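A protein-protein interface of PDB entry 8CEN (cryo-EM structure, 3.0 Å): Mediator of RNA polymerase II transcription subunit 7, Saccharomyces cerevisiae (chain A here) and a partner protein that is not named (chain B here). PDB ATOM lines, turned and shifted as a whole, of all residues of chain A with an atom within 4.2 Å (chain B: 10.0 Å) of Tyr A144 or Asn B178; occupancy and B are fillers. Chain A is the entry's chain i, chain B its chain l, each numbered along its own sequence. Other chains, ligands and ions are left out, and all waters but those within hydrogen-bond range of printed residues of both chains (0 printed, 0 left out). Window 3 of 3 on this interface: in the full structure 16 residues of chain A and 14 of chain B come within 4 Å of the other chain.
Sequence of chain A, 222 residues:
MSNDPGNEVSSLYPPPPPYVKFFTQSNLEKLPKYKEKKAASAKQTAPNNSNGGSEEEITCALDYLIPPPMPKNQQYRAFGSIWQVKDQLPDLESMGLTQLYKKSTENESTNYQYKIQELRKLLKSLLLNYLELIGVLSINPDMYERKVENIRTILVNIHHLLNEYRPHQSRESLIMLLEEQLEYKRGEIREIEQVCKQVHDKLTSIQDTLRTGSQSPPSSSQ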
ATOM      1  N   PRO A 141      -3.913  -6.272   3.616  1.00  0.00           N
ATOM      2  CA  PRO A 141      -4.546  -4.972   3.365  1.00  0.00           C
ATOM      3  C   PRO A 141      -3.622  -3.954   2.712  1.00  0.00           C
ATOM      4  O   PRO A 141      -3.529  -2.813   3.173  1.00  0.00           O
ATOM      5  CB  PRO A 141      -4.963  -4.523   4.767  1.00  0.00           C
ATOM      6  CG  PRO A 141      -3.895  -5.093   5.646  1.00  0.00           C
ATOM      7  CD  PRO A 141      -3.448  -6.395   5.009  1.00  0.00           C
ATOM      8  N   ASP A 142      -2.937  -4.351   1.637  1.00  0.00           N
ATOM      9  CA  ASP A 142      -2.103  -3.441   0.869  1.00  0.00           C
ATOM     10  C   ASP A 142      -2.468  -3.370  -0.605  1.00  0.00           C
ATOM     11  O   ASP A 142      -1.953  -2.490  -1.305  1.00  0.00           O
ATOM     12  CB  ASP A 142      -0.618  -3.817   1.007  1.00  0.00           C
ATOM     13  CG  ASP A 142      -0.156  -3.851   2.451  1.00  0.00           C
ATOM     14  OD1 ASP A 142      -0.574  -2.969   3.228  1.00  0.00           O
ATOM     15  OD2 ASP A 142       0.644  -4.741   2.805  1.00  0.00           O
ATOM     16  N   MET A 143      -3.318  -4.269  -1.106  1.00  0.00           N
ATOM     17  CA  MET A 143      -3.929  -4.112  -2.421  1.00  0.00           C
ATOM     18  C   MET A 143      -5.395  -3.707  -2.325  1.00  0.00           C
ATOM     19  O   MET A 143      -6.175  -3.970  -3.246  1.00  0.00           O
ATOM     20  CB  MET A 143      -3.786  -5.384  -3.259  1.00  0.00           C
ATOM     21  CG  MET A 143      -2.398  -5.590  -3.852  1.00  0.00           C
ATOM     22  SD  MET A 143      -1.168  -6.096  -2.646  1.00  0.00           S
ATOM     23  CE  MET A 143      -1.684  -7.794  -2.419  1.00  0.00           C
ATOM     24  N   TYR A 144      -5.781  -3.057  -1.224  1.00  0.00           N
ATOM     25  CA  TYR A 144      -7.162  -2.629  -1.039  1.00  0.00           C
ATOM     26  C   TYR A 144      -7.543  -1.476  -1.957  1.00  0.00           C
ATOM     27  O   TYR A 144      -8.738  -1.202  -2.113  1.00  0.00           O
ATOM     28  CB  TYR A 144      -7.390  -2.266   0.442  1.00  0.00           C
ATOM     29  CG  TYR A 144      -6.907  -0.892   0.906  1.00  0.00           C
ATOM     30  CD1 TYR A 144      -7.678   0.259   0.724  1.00  0.00           C
ATOM     31  CD2 TYR A 144      -5.677  -0.754   1.538  1.00  0.00           C
ATOM     32  CE1 TYR A 144      -7.229   1.497   1.142  1.00  0.00           C
ATOM     33  CE2 TYR A 144      -5.225   0.482   1.966  1.00  0.00           C
ATOM     34  CZ  TYR A 144      -6.006   1.601   1.766  1.00  0.00           C
ATOM     35  OH  TYR A 144      -5.557   2.831   2.189  1.00  0.00           O
ATOM     36  N   GLU A 145      -6.556  -0.784  -2.538  1.00  0.00           N
ATOM     37  CA  GLU A 145      -6.829   0.427  -3.305  1.00  0.00           C
ATOM     38  C   GLU A 145      -7.635   0.120  -4.560  1.00  0.00           C
ATOM     39  O   GLU A 145      -8.615   0.814  -4.858  1.00  0.00           O
ATOM     40  CB  GLU A 145      -5.516   1.122  -3.673  1.00  0.00           C
ATOM     41  CG  GLU A 145      -4.738   1.699  -2.494  1.00  0.00           C
ATOM     42  CD  GLU A 145      -3.886   0.664  -1.782  1.00  0.00           C
ATOM     43  OE1 GLU A 145      -3.848  -0.497  -2.243  1.00  0.00           O
ATOM     44  OE2 GLU A 145      -3.255   1.009  -0.760  1.00  0.00           O
ATOM     45  N   ARG A 146      -7.256  -0.930  -5.291  1.00  0.00           N
ATOM     46  CA  ARG A 146      -8.003  -1.293  -6.489  1.00  0.00           C
ATOM     47  C   ARG A 146      -9.394  -1.815  -6.154  1.00  0.00           C
ATOM     48  O   ARG A 146     -10.334  -1.558  -6.908  1.00  0.00           O
ATOM     49  CB  ARG A 146      -7.217  -2.310  -7.323  1.00  0.00           C
ATOM     50  CG  ARG A 146      -6.907  -3.623  -6.626  1.00  0.00           C
ATOM     51  CD  ARG A 146      -5.971  -4.486  -7.466  1.00  0.00           C
ATOM     52  NE  ARG A 146      -4.902  -3.715  -8.092  1.00  0.00           N
ATOM     53  CZ  ARG A 146      -3.814  -3.281  -7.468  1.00  0.00           C
ATOM     54  NH1 ARG A 146      -3.607  -3.524  -6.186  1.00  0.00           N
ATOM     55  NH2 ARG A 146      -2.909  -2.586  -8.152  1.00  0.00           N
ATOM     56  N   LYS A 147      -9.563  -2.509  -5.026  1.00  0.00           N
ATOM     57  CA  LYS A 147     -10.892  -2.999  -4.667  1.00  0.00           C
ATOM     58  C   LYS A 147     -11.810  -1.856  -4.246  1.00  0.00           C
ATOM     59  O   LYS A 147     -13.002  -1.850  -4.587  1.00  0.00           O
ATOM     60  CB  LYS A 147     -10.791  -4.049  -3.560  1.00  0.00           C
ATOM     61  CG  LYS A 147     -10.382  -5.442  -4.040  1.00  0.00           C
ATOM     62  CD  LYS A 147     -11.049  -5.836  -5.355  1.00  0.00           C
ATOM     63  CE  LYS A 147     -12.505  -6.234  -5.168  1.00  0.00           C
ATOM     64  NZ  LYS A 147     -13.143  -6.586  -6.466  1.00  0.00           N
ATOM     65  N   VAL A 148     -11.272  -0.878  -3.513  1.00  0.00           N
ATOM     66  CA  VAL A 148     -12.041   0.318  -3.177  1.00  0.00           C
ATOM     67  C   VAL A 148     -12.387   1.098  -4.441  1.00  0.00           C
ATOM     68  O   VAL A 148     -13.494   1.632  -4.574  1.00  0.00           O
ATOM     69  CB  VAL A 148     -11.272   1.174  -2.151  1.00  0.00           C
ATOM     70  CG1 VAL A 148     -11.920   2.538  -1.963  1.00  0.00           C
ATOM     71  CG2 VAL A 148     -11.215   0.456  -0.814  1.00  0.00           C
ATOM     72  N   PHE B 169       4.755  -2.568  11.718  1.00  0.00           N
ATOM     73  CA  PHE B 169       3.549  -2.930  12.457  1.00  0.00           C
ATOM     74  C   PHE B 169       2.587  -1.756  12.580  1.00  0.00           C
ATOM     75  O   PHE B 169       1.369  -1.938  12.486  1.00  0.00           O
ATOM     76  CB  PHE B 169       3.914  -3.458  13.841  1.00  0.00           C
ATOM     77  CG  PHE B 169       4.083  -4.941  13.886  1.00  0.00           C
ATOM     78  CD1 PHE B 169       3.050  -5.770  13.486  1.00  0.00           C
ATOM     79  CD2 PHE B 169       5.255  -5.508  14.353  1.00  0.00           C
ATOM     80  CE1 PHE B 169       3.194  -7.136  13.519  1.00  0.00           C
ATOM     81  CE2 PHE B 169       5.401  -6.878  14.397  1.00  0.00           C
ATOM     82  CZ  PHE B 169       4.367  -7.692  13.985  1.00  0.00           C
ATOM     83  N   ARG B 170       3.112  -0.552  12.818  1.00  0.00           N
ATOM     84  CA  ARG B 170       2.260   0.636  12.829  1.00  0.00           C
ATOM     85  C   ARG B 170       1.613   0.885  11.473  1.00  0.00           C
ATOM     86  O   ARG B 170       0.419   1.210  11.403  1.00  0.00           O
ATOM     87  CB  ARG B 170       3.057   1.858  13.285  1.00  0.00           C
ATOM     88  CG  ARG B 170       3.589   1.789  14.713  1.00  0.00           C
ATOM     89  CD  ARG B 170       2.478   2.032  15.760  1.00  0.00           C
ATOM     90  NE  ARG B 170       1.542   0.932  15.970  1.00  0.00           N
ATOM     91  CZ  ARG B 170       1.802  -0.155  16.682  1.00  0.00           C
ATOM     92  NH1 ARG B 170       2.967  -0.328  17.280  1.00  0.00           N
ATOM     93  NH2 ARG B 170       0.866  -1.093  16.800  1.00  0.00           N
ATOM     94  N   THR B 171       2.375   0.718  10.388  1.00  0.00           N
ATOM     95  CA  THR B 171       1.794   0.872   9.053  1.00  0.00           C
ATOM     96  C   THR B 171       0.679  -0.144   8.814  1.00  0.00           C
ATOM     97  O   THR B 171      -0.397   0.203   8.310  1.00  0.00           O
ATOM     98  CB  THR B 171       2.869   0.743   7.974  1.00  0.00           C
ATOM     99  OG1 THR B 171       3.457  -0.563   8.030  1.00  0.00           O
ATOM    100  CG2 THR B 171       3.941   1.808   8.143  1.00  0.00           C
ATOM    101  N   THR B 172       0.906  -1.402   9.202  1.00  0.00           N
ATOM    102  CA  THR B 172      -0.096  -2.434   8.955  1.00  0.00           C
ATOM    103  C   THR B 172      -1.316  -2.283   9.853  1.00  0.00           C
ATOM    104  O   THR B 172      -2.433  -2.602   9.432  1.00  0.00           O
ATOM    105  CB  THR B 172       0.515  -3.817   9.133  1.00  0.00           C
ATOM    106  OG1 THR B 172       1.168  -3.891  10.403  1.00  0.00           O
ATOM    107  CG2 THR B 172       1.522  -4.054   8.047  1.00  0.00           C
ATOM    108  N   ASN B 173      -1.131  -1.807  11.087  1.00  0.00           N
ATOM    109  CA  ASN B 173      -2.280  -1.529  11.939  1.00  0.00           C
ATOM    110  C   ASN B 173      -3.044  -0.306  11.458  1.00  0.00           C
ATOM    111  O   ASN B 173      -4.233  -0.162  11.763  1.00  0.00           O
ATOM    112  CB  ASN B 173      -1.833  -1.338  13.388  1.00  0.00           C
ATOM    113  CG  ASN B 173      -1.292  -2.610  14.004  1.00  0.00           C
ATOM    114  OD1 ASN B 173      -0.395  -2.570  14.844  1.00  0.00           O
ATOM    115  ND2 ASN B 173      -1.837  -3.749  13.592  1.00  0.00           N
ATOM    116  N   MET B 174      -2.387   0.584  10.718  1.00  0.00           N
ATOM    117  CA  MET B 174      -3.085   1.737  10.167  1.00  0.00           C
ATOM    118  C   MET B 174      -3.742   1.472   8.816  1.00  0.00           C
ATOM    119  O   MET B 174      -4.620   2.248   8.423  1.00  0.00           O
ATOM    120  CB  MET B 174      -2.116   2.921  10.042  1.00  0.00           C
ATOM    121  CG  MET B 174      -1.872   3.740  11.328  1.00  0.00           C
ATOM    122  SD  MET B 174      -3.184   4.233  12.498  1.00  0.00           S
ATOM    123  CE  MET B 174      -4.627   4.621  11.493  1.00  0.00           C
ATOM    124  N   ASN B 175      -3.339   0.414   8.100  1.00  0.00           N
ATOM    125  CA  ASN B 175      -3.905   0.164   6.769  1.00  0.00           C
ATOM    126  C   ASN B 175      -5.400  -0.149   6.810  1.00  0.00           C
ATOM    127  O   ASN B 175      -6.140   0.247   5.904  1.00  0.00           O
ATOM    128  CB  ASN B 175      -3.159  -0.967   6.057  1.00  0.00           C
ATOM    129  CG  ASN B 175      -1.719  -0.622   5.757  1.00  0.00           C
ATOM    130  OD1 ASN B 175      -0.828  -1.460   5.884  1.00  0.00           O
ATOM    131  ND2 ASN B 175      -1.481   0.620   5.352  1.00  0.00           N
ATOM    132  N   VAL B 176      -5.865  -0.867   7.836  1.00  0.00           N
ATOM    133  CA  VAL B 176      -7.280  -1.232   7.886  1.00  0.00           C
ATOM    134  C   VAL B 176      -8.143   0.002   8.134  1.00  0.00           C
ATOM    135  O   VAL B 176      -9.185   0.195   7.486  1.00  0.00           O
ATOM    136  CB  VAL B 176      -7.518  -2.316   8.951  1.00  0.00           C
ATOM    137  CG1 VAL B 176      -8.975  -2.755   8.950  1.00  0.00           C
ATOM    138  CG2 VAL B 176      -6.595  -3.502   8.722  1.00  0.00           C
ATOM    139  N   ASN B 177      -7.716   0.867   9.058  1.00  0.00           N
ATOM    140  CA  ASN B 177      -8.418   2.126   9.273  1.00  0.00           C
ATOM    141  C   ASN B 177      -8.318   3.035   8.056  1.00  0.00           C
ATOM    142  O   ASN B 177      -9.252   3.791   7.773  1.00  0.00           O
ATOM    143  CB  ASN B 177      -7.872   2.833  10.513  1.00  0.00           C
ATOM    144  CG  ASN B 177      -8.931   3.651  11.232  1.00  0.00           C
ATOM    145  OD1 ASN B 177      -9.929   4.054  10.637  1.00  0.00           O
ATOM    146  ND2 ASN B 177      -8.716   3.894  12.518  1.00  0.00           N
ATOM    147  N   ASN B 178      -7.205   2.968   7.318  1.00  0.00           N
ATOM    148  CA  ASN B 178      -7.095   3.722   6.074  1.00  0.00           C
ATOM    149  C   ASN B 178      -8.090   3.227   5.033  1.00  0.00           C
ATOM    150  O   ASN B 178      -8.671   4.027   4.294  1.00  0.00           O
ATOM    151  CB  ASN B 178      -5.667   3.643   5.536  1.00  0.00           C
ATOM    152  CG  ASN B 178      -4.703   4.500   6.328  1.00  0.00           C
ATOM    153  OD1 ASN B 178      -5.079   5.536   6.877  1.00  0.00           O
ATOM    154  ND2 ASN B 178      -3.451   4.064   6.402  1.00  0.00           N
ATOM    155  N   CYS B 179      -8.294   1.910   4.953  1.00  0.00           N
ATOM    156  CA  CYS B 179      -9.306   1.362   4.050  1.00  0.00           C
ATOM    157  C   CYS B 179     -10.706   1.798   4.463  1.00  0.00           C
ATOM    158  O   CYS B 179     -11.551   2.104   3.610  1.00  0.00           O
ATOM    159  CB  CYS B 179      -9.208  -0.162   4.011  1.00  0.00           C
ATOM    160  SG  CYS B 179     -10.438  -0.962   2.953  1.00  0.00           S
ATOM    161  N   ILE B 180     -10.963   1.832   5.772  1.00  0.00           N
ATOM    162  CA  ILE B 180     -12.252   2.303   6.280  1.00  0.00           C
ATOM    163  C   ILE B 180     -12.474   3.768   5.912  1.00  0.00           C
ATOM    164  O   ILE B 180     -13.555   4.155   5.451  1.00  0.00           O
ATOM    165  CB  ILE B 180     -12.334   2.079   7.800  1.00  0.00           C
ATOM    166  CG1 ILE B 180     -12.533   0.595   8.102  1.00  0.00           C
ATOM    167  CG2 ILE B 180     -13.442   2.912   8.414  1.00  0.00           C
ATOM    168  CD1 ILE B 180     -12.302   0.244   9.540  1.00  0.00           C
ATOM    169  N   TRP B 181     -11.447   4.602   6.094  1.00  0.00           N
ATOM    170  CA  TRP B 181     -11.563   6.014   5.741  1.00  0.00           C
ATOM    171  C   TRP B 181     -11.648   6.219   4.233  1.00  0.00           C
ATOM    172  O   TRP B 181     -12.263   7.187   3.778  1.00  0.00           O
ATOM    173  CB  TRP B 181     -10.389   6.801   6.327  1.00  0.00           C
ATOM    174  CG  TRP B 181     -10.533   7.089   7.798  1.00  0.00           C
ATOM    175  CD1 TRP B 181      -9.736   6.628   8.803  1.00  0.00           C
ATOM    176  CD2 TRP B 181     -11.517   7.927   8.421  1.00  0.00           C
ATOM    177  NE1 TRP B 181     -10.172   7.107  10.013  1.00  0.00           N
ATOM    178  CE2 TRP B 181     -11.262   7.910   9.806  1.00  0.00           C
ATOM    179  CE3 TRP B 181     -12.591   8.686   7.944  1.00  0.00           C
ATOM    180  CZ2 TRP B 181     -12.040   8.620  10.719  1.00  0.00           C
ATOM    181  CZ3 TRP B 181     -13.361   9.391   8.852  1.00  0.00           C
ATOM    182  CH2 TRP B 181     -13.083   9.351  10.223  1.00  0.00           C
ATOM    183  N   ALA B 182     -11.053   5.320   3.444  1.00  0.00           N
ATOM    184  CA  ALA B 182     -11.226   5.368   1.995  1.00  0.00           C
ATOM    185  C   ALA B 182     -12.667   5.066   1.606  1.00  0.00           C
ATOM    186  O   ALA B 182     -13.234   5.727   0.724  1.00  0.00           O
ATOM    187  CB  ALA B 182     -10.266   4.391   1.319  1.00  0.00           C
ATOM    188  N   LEU B 183     -13.278   4.077   2.262  1.00  0.00           N
ATOM    189  CA  LEU B 183     -14.696   3.811   2.042  1.00  0.00           C
ATOM    190  C   LEU B 183     -15.564   4.973   2.513  1.00  0.00           C
ATOM    191  O   LEU B 183     -16.597   5.262   1.900  1.00  0.00           O
ATOM    192  CB  LEU B 183     -15.107   2.517   2.744  1.00  0.00           C
ATOM    193  CG  LEU B 183     -15.025   1.251   1.888  1.00  0.00           C
ATOM    194  CD1 LEU B 183     -15.404   0.031   2.703  1.00  0.00           C
ATOM    195  CD2 LEU B 183     -15.908   1.369   0.653  1.00  0.00           C
ATOM    196  N   LYS B 184     -15.157   5.657   3.585  1.00  0.00           N
ATOM    197  CA  LYS B 184     -15.894   6.834   4.039  1.00  0.00           C
ATOM    198  C   LYS B 184     -15.772   7.990   3.051  1.00  0.00           C
ATOM    199  O   LYS B 184     -16.730   8.744   2.855  1.00  0.00           O
ATOM    200  CB  LYS B 184     -15.414   7.264   5.424  1.00  0.00           C
ATOM    201  CG  LYS B 184     -16.093   6.523   6.554  1.00  0.00           C
ATOM    202  CD  LYS B 184     -16.065   7.311   7.849  1.00  0.00           C
ATOM    203  CE  LYS B 184     -17.076   6.764   8.844  1.00  0.00           C
ATOM    204  NZ  LYS B 184     -16.969   7.426  10.173  1.00  0.00           N
ATOM    205  N   SER B 185     -14.600   8.158   2.435  1.00  0.00           N
ATOM    206  CA  SER B 185     -14.449   9.180   1.403  1.00  0.00           C
ATOM    207  C   SER B 185     -15.277   8.836   0.171  1.00  0.00           C
ATOM    208  O   SER B 185     -15.841   9.726  -0.476  1.00  0.00           O
ATOM    209  CB  SER B 185     -12.977   9.345   1.028  1.00  0.00           C
ATOM    210  OG  SER B 185     -12.408   8.106   0.653  1.00  0.00           O
ATOM    211  N   SER B 186     -15.367   7.543  -0.156  1.00  0.00           N
ATOM    212  CA  SER B 186     -16.256   7.108  -1.231  1.00  0.00           C
ATOM    213  C   SER B 186     -17.716   7.379  -0.882  1.00  0.00           C
ATOM    214  O   SER B 186     -18.520   7.710  -1.762  1.00  0.00           O
ATOM    215  CB  SER B 186     -16.036   5.625  -1.517  1.00  0.00           C
ATOM    216  OG  SER B 186     -14.682   5.370  -1.854  1.00  0.00           O
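OD1 of Asn B175 lies close to OD1 of Asp A142.
ND2 of Asn B178 is in hydrogen-bond range of O of Met B174 (3.0 Å).
O of Ala B182 sits at hydrogen-bond distance from OG of Ser B186, at 3.0 Å.
The side-chain amide oxygen (OD1) of Asn B175 sits close to the backbone carbonyl oxygen (O) of Thr B171 (3.0 Å).
Pro A141 touches Asn B175.
Tyr A144 touches Asn B178.
Tyr A144 touches Cys B179.
CG1 of Val A148 touches OG of Ser B186, at 3.96 Å.
Of chain B, only Asn B178 (3.4 Å) and Cys B179 (3.6 Å) come within 4 Å of Tyr A144.
Asn B178 touches just one residue of chain A: Tyr A144.
No residue of chain B comes within 4 Å of Glu A145.
Of the printed residues of chain A, Cys B179 touches Tyr A144.
Of the printed residues of chain A, Ser B186 touches Val A148 (3.96 Å).
Of the printed residues of chain B, Asp A142 touches Asn B175.
Of the printed residues of chain B, Pro A141 touches Asn B175 (3.4 Å).
Val B176 touches none of the printed residues of chain A.
Ser B185 touches none of the printed residues of chain A.
The nearest printed residue of chain A that does not touch Asn B178 is Val A148 (6.7 Å).
Printed residues of chain A that touch a printed residue of chain B: Pro A141, Asp A142, Tyr A144 and Val A148.
Hydrophobic or aromatic side chains of chain A within 4 Å of the printed part of chain B: Tyr A144 and Val A148.
Among the printed residues, no Asp or Glu carboxylate lies within 4 Å of a Lys or Arg side-chain nitrogen of the other chain.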
